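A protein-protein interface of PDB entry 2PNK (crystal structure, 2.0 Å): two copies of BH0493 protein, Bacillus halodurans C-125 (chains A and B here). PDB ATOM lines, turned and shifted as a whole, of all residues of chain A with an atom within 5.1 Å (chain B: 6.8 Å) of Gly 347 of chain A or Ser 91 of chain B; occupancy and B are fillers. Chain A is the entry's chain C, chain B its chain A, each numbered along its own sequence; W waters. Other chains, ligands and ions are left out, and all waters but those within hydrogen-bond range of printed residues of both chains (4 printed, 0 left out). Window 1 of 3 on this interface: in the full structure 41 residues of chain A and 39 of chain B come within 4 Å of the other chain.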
ATOM      1  N   ARG A 342     -22.731  -9.519   0.592  1.00  0.00           N
ATOM      2  CA  ARG A 342     -24.149  -9.272   0.655  1.00  0.00           C
ATOM      3  C   ARG A 342     -24.822  -9.615  -0.662  1.00  0.00           C
ATOM      4  O   ARG A 342     -25.839 -10.282  -0.665  1.00  0.00           O
ATOM      5  CB  ARG A 342     -24.407  -7.804   1.014  1.00  0.00           C
ATOM      6  CG  ARG A 342     -24.304  -7.511   2.512  1.00  0.00           C
ATOM      7  CD  ARG A 342     -24.219  -6.041   2.773  1.00  0.00           C
ATOM      8  NE  ARG A 342     -24.396  -5.714   4.176  1.00  0.00           N
ATOM      9  CZ  ARG A 342     -24.693  -4.492   4.615  1.00  0.00           C
ATOM     10  NH1 ARG A 342     -24.791  -3.488   3.770  1.00  0.00           N
ATOM     11  NH2 ARG A 342     -24.893  -4.274   5.910  1.00  0.00           N
ATOM     12  N   MET A 343     -24.264  -9.133  -1.777  1.00  0.00           N
ATOM     13  CA  MET A 343     -24.852  -9.435  -3.073  1.00  0.00           C
ATOM     14  C   MET A 343     -24.746 -10.914  -3.437  1.00  0.00           C
ATOM     15  O   MET A 343     -25.671 -11.491  -4.035  1.00  0.00           O
ATOM     16  CB  MET A 343     -24.245  -8.578  -4.165  1.00  0.00           C
ATOM     17  CG  MET A 343     -25.001  -8.703  -5.491  1.00  0.00           C
ATOM     18  SD  MET A 343     -24.654  -7.199  -6.663  1.00  0.00           S
ATOM     19  CE  MET A 343     -25.590  -5.843  -5.572  1.00  0.00           C
ATOM     20  N   GLU A 344     -23.623 -11.521  -3.074  1.00  0.00           N
ATOM     21  CA  GLU A 344     -23.412 -12.920  -3.369  1.00  0.00           C
ATOM     22  C   GLU A 344     -24.451 -13.837  -2.703  1.00  0.00           C
ATOM     23  O   GLU A 344     -24.884 -14.848  -3.281  1.00  0.00           O
ATOM     24  CB  GLU A 344     -21.949 -13.304  -3.011  1.00  0.00           C
ATOM     25  CG  GLU A 344     -20.989 -12.972  -4.140  1.00  0.00           C
ATOM     26  CD  GLU A 344     -19.510 -12.866  -3.763  1.00  0.00           C
ATOM     27  OE1 GLU A 344     -19.089 -13.430  -2.725  1.00  0.00           O
ATOM     28  OE2 GLU A 344     -18.747 -12.247  -4.552  1.00  0.00           O
ATOM     29  N   MET A 345     -24.839 -13.511  -1.484  1.00  0.00           N
ATOM     30  CA  MET A 345     -25.733 -14.373  -0.725  1.00  0.00           C
ATOM     31  C   MET A 345     -27.164 -13.836  -0.706  1.00  0.00           C
ATOM     32  O   MET A 345     -28.071 -14.586  -0.427  1.00  0.00           O
ATOM     33  CB  MET A 345     -25.212 -14.547   0.703  1.00  0.00           C
ATOM     34  CG  MET A 345     -24.273 -15.712   0.928  1.00  0.00           C
ATOM     35  SD  MET A 345     -23.732 -15.720   2.795  1.00  0.00           S
ATOM     36  CE  MET A 345     -22.566 -14.252   2.669  1.00  0.00           C
ATOM     37  N   LEU A 346     -27.388 -12.559  -1.027  1.00  0.00           N
ATOM     38  CA  LEU A 346     -28.763 -12.001  -1.014  1.00  0.00           C
ATOM     39  C   LEU A 346     -29.236 -11.417  -2.353  1.00  0.00           C
ATOM     40  O   LEU A 346     -30.383 -10.942  -2.453  1.00  0.00           O
ATOM     41  CB  LEU A 346     -28.873 -10.902   0.049  1.00  0.00           C
ATOM     42  CG  LEU A 346     -28.551 -11.260   1.505  1.00  0.00           C
ATOM     43  CD1 LEU A 346     -28.577  -9.959   2.439  1.00  0.00           C
ATOM     44  CD2 LEU A 346     -29.520 -12.346   2.076  1.00  0.00           C
ATOM     45  N   GLY A 347     -28.388 -11.433  -3.379  1.00  0.00           N
ATOM     46  CA  GLY A 347     -28.737 -10.817  -4.665  1.00  0.00           C
ATOM     47  C   GLY A 347     -29.071  -9.344  -4.458  1.00  0.00           C
ATOM     48  O   GLY A 347     -28.255  -8.574  -3.979  1.00  0.00           O
ATOM     49  N   THR A 348     -30.264  -8.903  -4.816  1.00  0.00           N
ATOM     50  CA  THR A 348     -30.515  -7.474  -4.666  1.00  0.00           C
ATOM     51  C   THR A 348     -31.408  -7.171  -3.470  1.00  0.00           C
ATOM     52  O   THR A 348     -31.898  -6.049  -3.349  1.00  0.00           O
ATOM     53  CB  THR A 348     -31.065  -6.874  -5.953  1.00  0.00           C
ATOM     54  OG1 THR A 348     -32.306  -7.519  -6.315  1.00  0.00           O
ATOM     55  CG2 THR A 348     -30.008  -6.984  -7.098  1.00  0.00           C
ATOM     56  N   SER A 349     -31.622  -8.154  -2.586  1.00  0.00           N
ATOM     57  CA  SER A 349     -32.602  -7.988  -1.498  1.00  0.00           C
ATOM     58  C   SER A 349     -31.991  -7.335  -0.244  1.00  0.00           C
ATOM     59  O   SER A 349     -32.130  -7.860   0.849  1.00  0.00           O
ATOM     60  CB  SER A 349     -33.337  -9.311  -1.154  1.00  0.00           C
ATOM     61  OG  SER A 349     -32.446 -10.301  -0.656  1.00  0.00           O
ATOM     62  N   PHE A 350     -31.352  -6.168  -0.411  1.00  0.00           N
ATOM     63  CA  PHE A 350     -30.760  -5.432   0.725  1.00  0.00           C
ATOM     64  C   PHE A 350     -30.582  -3.950   0.356  1.00  0.00           C
ATOM     65  O   PHE A 350     -30.843  -3.541  -0.792  1.00  0.00           O
ATOM     66  CB  PHE A 350     -29.438  -6.098   1.197  1.00  0.00           C
ATOM     67  CG  PHE A 350     -28.282  -5.914   0.261  1.00  0.00           C
ATOM     68  CD1 PHE A 350     -28.162  -6.702  -0.881  1.00  0.00           C
ATOM     69  CD2 PHE A 350     -27.308  -4.960   0.516  1.00  0.00           C
ATOM     70  CE1 PHE A 350     -27.110  -6.519  -1.778  1.00  0.00           C
ATOM     71  CE2 PHE A 350     -26.229  -4.781  -0.378  1.00  0.00           C
ATOM     72  CZ  PHE A 350     -26.130  -5.553  -1.510  1.00  0.00           C
ATOM     73  N   LEU B  52     -31.765 -21.359  -2.881  1.00  0.00           N
ATOM     74  CA  LEU B  52     -32.679 -20.501  -3.607  1.00  0.00           C
ATOM     75  C   LEU B  52     -34.040 -20.330  -2.908  1.00  0.00           C
ATOM     76  O   LEU B  52     -34.706 -19.321  -3.132  1.00  0.00           O
ATOM     77  CB  LEU B  52     -32.871 -21.022  -5.037  1.00  0.00           C
ATOM     78  CG  LEU B  52     -31.595 -21.102  -5.884  1.00  0.00           C
ATOM     79  CD1 LEU B  52     -31.895 -21.672  -7.229  1.00  0.00           C
ATOM     80  CD2 LEU B  52     -30.971 -19.750  -6.040  1.00  0.00           C
ATOM     81  N   GLU B  55     -33.548 -17.537  -0.632  1.00  0.00           N
ATOM     82  CA  GLU B  55     -33.527 -16.288  -1.369  1.00  0.00           C
ATOM     83  C   GLU B  55     -34.925 -15.900  -1.875  1.00  0.00           C
ATOM     84  O   GLU B  55     -35.284 -14.718  -1.849  1.00  0.00           O
ATOM     85  CB  GLU B  55     -32.516 -16.358  -2.524  1.00  0.00           C
ATOM     86  CG  GLU B  55     -31.079 -16.304  -2.048  1.00  0.00           C
ATOM     87  CD  GLU B  55     -30.041 -16.476  -3.165  1.00  0.00           C
ATOM     88  OE1 GLU B  55     -30.277 -16.006  -4.311  1.00  0.00           O
ATOM     89  OE2 GLU B  55     -28.976 -17.060  -2.866  1.00  0.00           O
ATOM     90  N   TRP B  59     -38.341 -12.251  -1.104  1.00  0.00           N
ATOM     91  CA  TRP B  59     -38.978 -11.446  -2.140  1.00  0.00           C
ATOM     92  C   TRP B  59     -40.472 -11.733  -2.276  1.00  0.00           C
ATOM     93  O   TRP B  59     -41.272 -10.804  -2.411  1.00  0.00           O
ATOM     94  CB  TRP B  59     -38.292 -11.736  -3.487  1.00  0.00           C
ATOM     95  CG  TRP B  59     -37.034 -10.957  -3.765  1.00  0.00           C
ATOM     96  CD1 TRP B  59     -35.761 -11.467  -4.063  1.00  0.00           C
ATOM     97  CD2 TRP B  59     -36.924  -9.538  -3.823  1.00  0.00           C
ATOM     98  NE1 TRP B  59     -34.890 -10.414  -4.273  1.00  0.00           N
ATOM     99  CE2 TRP B  59     -35.577  -9.226  -4.130  1.00  0.00           C
ATOM    100  CE3 TRP B  59     -37.841  -8.485  -3.627  1.00  0.00           C
ATOM    101  CZ2 TRP B  59     -35.130  -7.916  -4.270  1.00  0.00           C
ATOM    102  CZ3 TRP B  59     -37.392  -7.183  -3.763  1.00  0.00           C
ATOM    103  CH2 TRP B  59     -36.033  -6.913  -4.075  1.00  0.00           C
ATOM    104  N   LEU B  83     -36.660 -14.570  -8.809  1.00  0.00           N
ATOM    105  CA  LEU B  83     -35.207 -14.374  -8.651  1.00  0.00           C
ATOM    106  C   LEU B  83     -34.429 -14.168  -9.973  1.00  0.00           C
ATOM    107  O   LEU B  83     -33.323 -13.632  -9.940  1.00  0.00           O
ATOM    108  CB  LEU B  83     -34.576 -15.560  -7.880  1.00  0.00           C
ATOM    109  CG  LEU B  83     -35.009 -15.854  -6.445  1.00  0.00           C
ATOM    110  CD1 LEU B  83     -34.137 -16.984  -5.856  1.00  0.00           C
ATOM    111  CD2 LEU B  83     -34.942 -14.605  -5.587  1.00  0.00           C
ATOM    112  N   SER B  88     -32.522  -9.217 -11.320  1.00  0.00           N
ATOM    113  CA  SER B  88     -31.466  -9.903 -12.061  1.00  0.00           C
ATOM    114  C   SER B  88     -30.875 -11.000 -11.177  1.00  0.00           C
ATOM    115  O   SER B  88     -30.781 -10.818  -9.970  1.00  0.00           O
ATOM    116  CB  SER B  88     -30.399  -8.930 -12.522  1.00  0.00           C
ATOM    117  OG  SER B  88     -30.996  -8.014 -13.424  1.00  0.00           O
ATOM    118  N   PRO B  89     -30.564 -12.172 -11.763  1.00  0.00           N
ATOM    119  CA  PRO B  89     -30.098 -13.312 -11.004  1.00  0.00           C
ATOM    120  C   PRO B  89     -28.596 -13.217 -10.648  1.00  0.00           C
ATOM    121  O   PRO B  89     -27.782 -14.038 -11.074  1.00  0.00           O
ATOM    122  CB  PRO B  89     -30.453 -14.494 -11.918  1.00  0.00           C
ATOM    123  CG  PRO B  89     -30.376 -13.947 -13.265  1.00  0.00           C
ATOM    124  CD  PRO B  89     -30.703 -12.495 -13.194  1.00  0.00           C
ATOM    125  N   VAL B  90     -28.252 -12.195  -9.873  1.00  0.00           N
ATOM    126  CA  VAL B  90     -26.850 -11.876  -9.584  1.00  0.00           C
ATOM    127  C   VAL B  90     -26.224 -12.651  -8.419  1.00  0.00           C
ATOM    128  O   VAL B  90     -24.981 -12.730  -8.335  1.00  0.00           O
ATOM    129  CB  VAL B  90     -26.626 -10.370  -9.371  1.00  0.00           C
ATOM    130  CG1 VAL B  90     -26.747  -9.635 -10.713  1.00  0.00           C
ATOM    131  CG2 VAL B  90     -27.590  -9.783  -8.308  1.00  0.00           C
ATOM    132  N   SER B  91     -27.047 -13.267  -7.565  1.00  0.00           N
ATOM    133  CA  SER B  91     -26.533 -14.029  -6.418  1.00  0.00           C
ATOM    134  C   SER B  91     -25.715 -15.206  -6.903  1.00  0.00           C
ATOM    135  O   SER B  91     -25.909 -15.668  -8.012  1.00  0.00           O
ATOM    136  CB  SER B  91     -27.687 -14.536  -5.532  1.00  0.00           C
ATOM    137  OG  SER B  91     -28.371 -15.637  -6.110  1.00  0.00           O
ATOM    138  N   GLU B  92     -24.815 -15.704  -6.058  1.00  0.00           N
ATOM    139  CA  GLU B  92     -23.982 -16.827  -6.433  1.00  0.00           C
ATOM    140  C   GLU B  92     -24.803 -18.063  -6.793  1.00  0.00           C
ATOM    141  O   GLU B  92     -24.505 -18.748  -7.778  1.00  0.00           O
ATOM    142  CB  GLU B  92     -22.939 -17.101  -5.334  1.00  0.00           C
ATOM    143  CG  GLU B  92     -22.077 -18.284  -5.562  1.00  0.00           C
ATOM    144  CD  GLU B  92     -21.224 -18.194  -6.791  1.00  0.00           C
ATOM    145  OE1 GLU B  92     -21.050 -17.102  -7.399  1.00  0.00           O
ATOM    146  OE2 GLU B  92     -20.724 -19.253  -7.133  1.00  0.00           O
ATOM    147  N   ALA B  93     -25.851 -18.329  -6.024  1.00  0.00           N
ATOM    148  CA  ALA B  93     -26.712 -19.485  -6.248  1.00  0.00           C
ATOM    149  C   ALA B  93     -27.482 -19.404  -7.578  1.00  0.00           C
ATOM    150  O   ALA B  93     -27.561 -20.393  -8.318  1.00  0.00           O
ATOM    151  CB  ALA B  93     -27.689 -19.667  -5.063  1.00  0.00           C
ATOM    152  N   CYS B  94     -28.002 -18.216  -7.880  1.00  0.00           N
ATOM    153  CA  CYS B  94     -28.683 -17.954  -9.114  1.00  0.00           C
ATOM    154  C   CYS B  94     -27.772 -18.031 -10.327  1.00  0.00           C
ATOM    155  O   CYS B  94     -28.083 -18.715 -11.305  1.00  0.00           O
ATOM    156  CB  CYS B  94     -29.330 -16.570  -9.035  1.00  0.00           C
ATOM    157  SG  CYS B  94     -30.845 -16.538  -7.964  1.00  0.00           S
ATOM    158  N   ARG B  95     -26.645 -17.326 -10.258  1.00  0.00           N
ATOM    159  CA  ARG B  95     -25.590 -17.415 -11.265  1.00  0.00           C
ATOM    160  C   ARG B  95     -25.245 -18.877 -11.536  1.00  0.00           C
ATOM    161  O   ARG B  95     -25.080 -19.263 -12.673  1.00  0.00           O
ATOM    162  CB  ARG B  95     -24.350 -16.670 -10.753  1.00  0.00           C
ATOM    163  CG  ARG B  95     -23.104 -16.677 -11.652  1.00  0.00           C
ATOM    164  CD  ARG B  95     -21.866 -16.401 -10.809  1.00  0.00           C
ATOM    165  NE  ARG B  95     -20.642 -16.618 -11.563  1.00  0.00           N
ATOM    166  CZ  ARG B  95     -19.440 -16.841 -11.035  1.00  0.00           C
ATOM    167  NH1 ARG B  95     -19.250 -16.870  -9.730  1.00  0.00           N
ATOM    168  NH2 ARG B  95     -18.406 -17.045 -11.833  1.00  0.00           N
ATOM    169  N   GLY B  96     -25.125 -19.684 -10.477  1.00  0.00           N
ATOM    170  CA  GLY B  96     -24.728 -21.065 -10.625  1.00  0.00           C
ATOM    171  C   GLY B  96     -25.686 -21.818 -11.529  1.00  0.00           C
ATOM    172  O   GLY B  96     -25.256 -22.620 -12.372  1.00  0.00           O
ATOM    173  N   ASN B 331     -18.723 -18.590  -1.560  1.00  0.00           N
ATOM    174  CA  ASN B 331     -19.084 -17.357  -2.231  1.00  0.00           C
ATOM    175  C   ASN B 331     -17.787 -16.710  -2.717  1.00  0.00           C
ATOM    176  O   ASN B 331     -16.802 -16.706  -1.983  1.00  0.00           O
ATOM    177  CB  ASN B 331     -19.805 -16.463  -1.222  1.00  0.00           C
ATOM    178  CG  ASN B 331     -21.197 -16.974  -0.931  1.00  0.00           C
ATOM    179  OD1 ASN B 331     -22.026 -17.003  -1.826  1.00  0.00           O
ATOM    180  ND2 ASN B 331     -21.435 -17.462   0.284  1.00  0.00           N
ATOM    181  N   HIS B 369     -16.929 -22.143 -11.287  1.00  0.00           N
ATOM    182  CA  HIS B 369     -16.764 -20.940 -10.487  1.00  0.00           C
ATOM    183  C   HIS B 369     -15.524 -20.982  -9.601  1.00  0.00           C
ATOM    184  O   HIS B 369     -14.757 -20.026  -9.533  1.00  0.00           O
ATOM    185  CB  HIS B 369     -17.966 -20.691  -9.581  1.00  0.00           C
ATOM    186  CG  HIS B 369     -19.230 -20.355 -10.312  1.00  0.00           C
ATOM    187  ND1 HIS B 369     -20.373 -19.945  -9.664  1.00  0.00           N
ATOM    188  CD2 HIS B 369     -19.534 -20.380 -11.634  1.00  0.00           C
ATOM    189  CE1 HIS B 369     -21.339 -19.770 -10.550  1.00  0.00           C
ATOM    190  NE2 HIS B 369     -20.862 -20.047 -11.752  1.00  0.00           N
HETATM  191  O   HOH W   1     -26.336 -17.139  -3.413  1.00  0.00           O
HETATM  192  O   HOH W   2     -33.046 -12.762  -1.801  1.00  0.00           O
HETATM  193  O   HOH W   3     -32.258 -11.080  -5.593  1.00  0.00           O
HETATM  194  O   HOH W   4     -31.191 -13.560  -4.276  1.00  0.00           O
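The backbone carbonyl oxygen (O) of Glu 344 of chain A is in hydrogen-bond range of the backbone NH (N) of Glu 92 of chain B, at 2.9 Å.
OE1 of Glu 55 of chain B sits at hydrogen-bond distance from OG of Ser 91 of chain B (2.6 Å). The side-chain carboxylate (OE1) of Glu 55 of chain B lies within hydrogen-bond range of the side-chain sulfur (SG) of Cys 94 of chain B (3.7 Å). N of Cys 94 of chain B is in hydrogen-bond range of OG of Ser 91 of chain B, 3.1 Å away. OE1 of Glu 92 of chain B is in salt-bridge range of NH1 of Arg 95 of chain B, at 3.0 Å. ND1 of His 369 of chain B is in hydrogen-bond range of OE2 of Glu 92 of chain B (2.6 Å). O of Leu 346 of chain A lies within hydrogen-bond range of OG of Ser 349 of chain A.
Among the printed residues, merely in contact across the chains: Met 345 of chain A with Asn 331 of chain B (3.4 Å), Glu 344 of chain A with Asn 331 of chain B (3.5 Å), Thr 348 of chain A with Trp 59 of chain B (3.5 Å), Met 343 of chain A with Ser 91 of chain B (3.6 Å), Met 345 of chain A with Glu 55 of chain B (3.6 Å), Glu 344 of chain A with Ser 91 of chain B (3.6 Å), Ser 349 of chain A with Trp 59 of chain B (3.7 Å), Gly 347 of chain A with Ser 91 of chain B (3.8 Å), Thr 348 of chain A with Val 90 of chain B (3.9 Å), Gly 347 of chain A with Val 90 of chain B (3.96 Å) and Met 343 of chain A with Val 90 of chain B (3.98 Å).
Of the printed residues of chain B, Met 345 of chain A touches Glu 55 and Asn 331. Gly 347 of chain A touches just these residues of chain B: Val 90 (3.96 Å) and Ser 91 (3.8 Å). Printed residues of chain B within 4 Å of Ser 349 of chain A: Trp 59 (3.7 Å). Ser 91 of chain B touches just these residues of chain A: Met 343, Glu 344 and Gly 347. The nearest residue of chain A that does not touch Ser 91 of chain B is Leu 346 of chain A (4.7 Å). The nearest printed residue of chain B that does not touch Thr 348 of chain A is Ser 88 of chain B (4.9 Å).
Of the 9 printed residues of chain A, 6 touch a printed residue of chain B. Along chain A the printed residues that touch a printed residue of chain B span positions 343 to 349. Of the 15 printed residues of chain B, 6 touch a printed residue of chain A. Hydrophobic or aromatic side chains of chain B that line the printed part of chain A: Trp 59 and Val 90.
No position is printed for both chains.
Water W4 lies within hydrogen-bond range of the side-chain carboxylate of Glu 55 of chain B (2.6 Å) and the backbone carbonyl oxygen of Leu 346 of chain A (3.3 Å). Water W1 lies within hydrogen-bond range of OE2 of Glu 55 of chain B (2.7 Å), O of Glu 344 of chain A (2.7 Å), N of Ala 93 of chain B (2.9 Å) and N of Glu 92 of chain B (3.4 Å). Water W2 lies within hydrogen-bond range of OG of Ser 349 of chain A (2.8 Å), O of Glu 55 of chain B (3.0 Å) and O of Leu 346 of chain A (3.3 Å). Water W3 lies within hydrogen-bond range of NE1 of Trp 59 of chain B (3.0 Å) and N of Thr 348 of chain A (3.1 Å).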
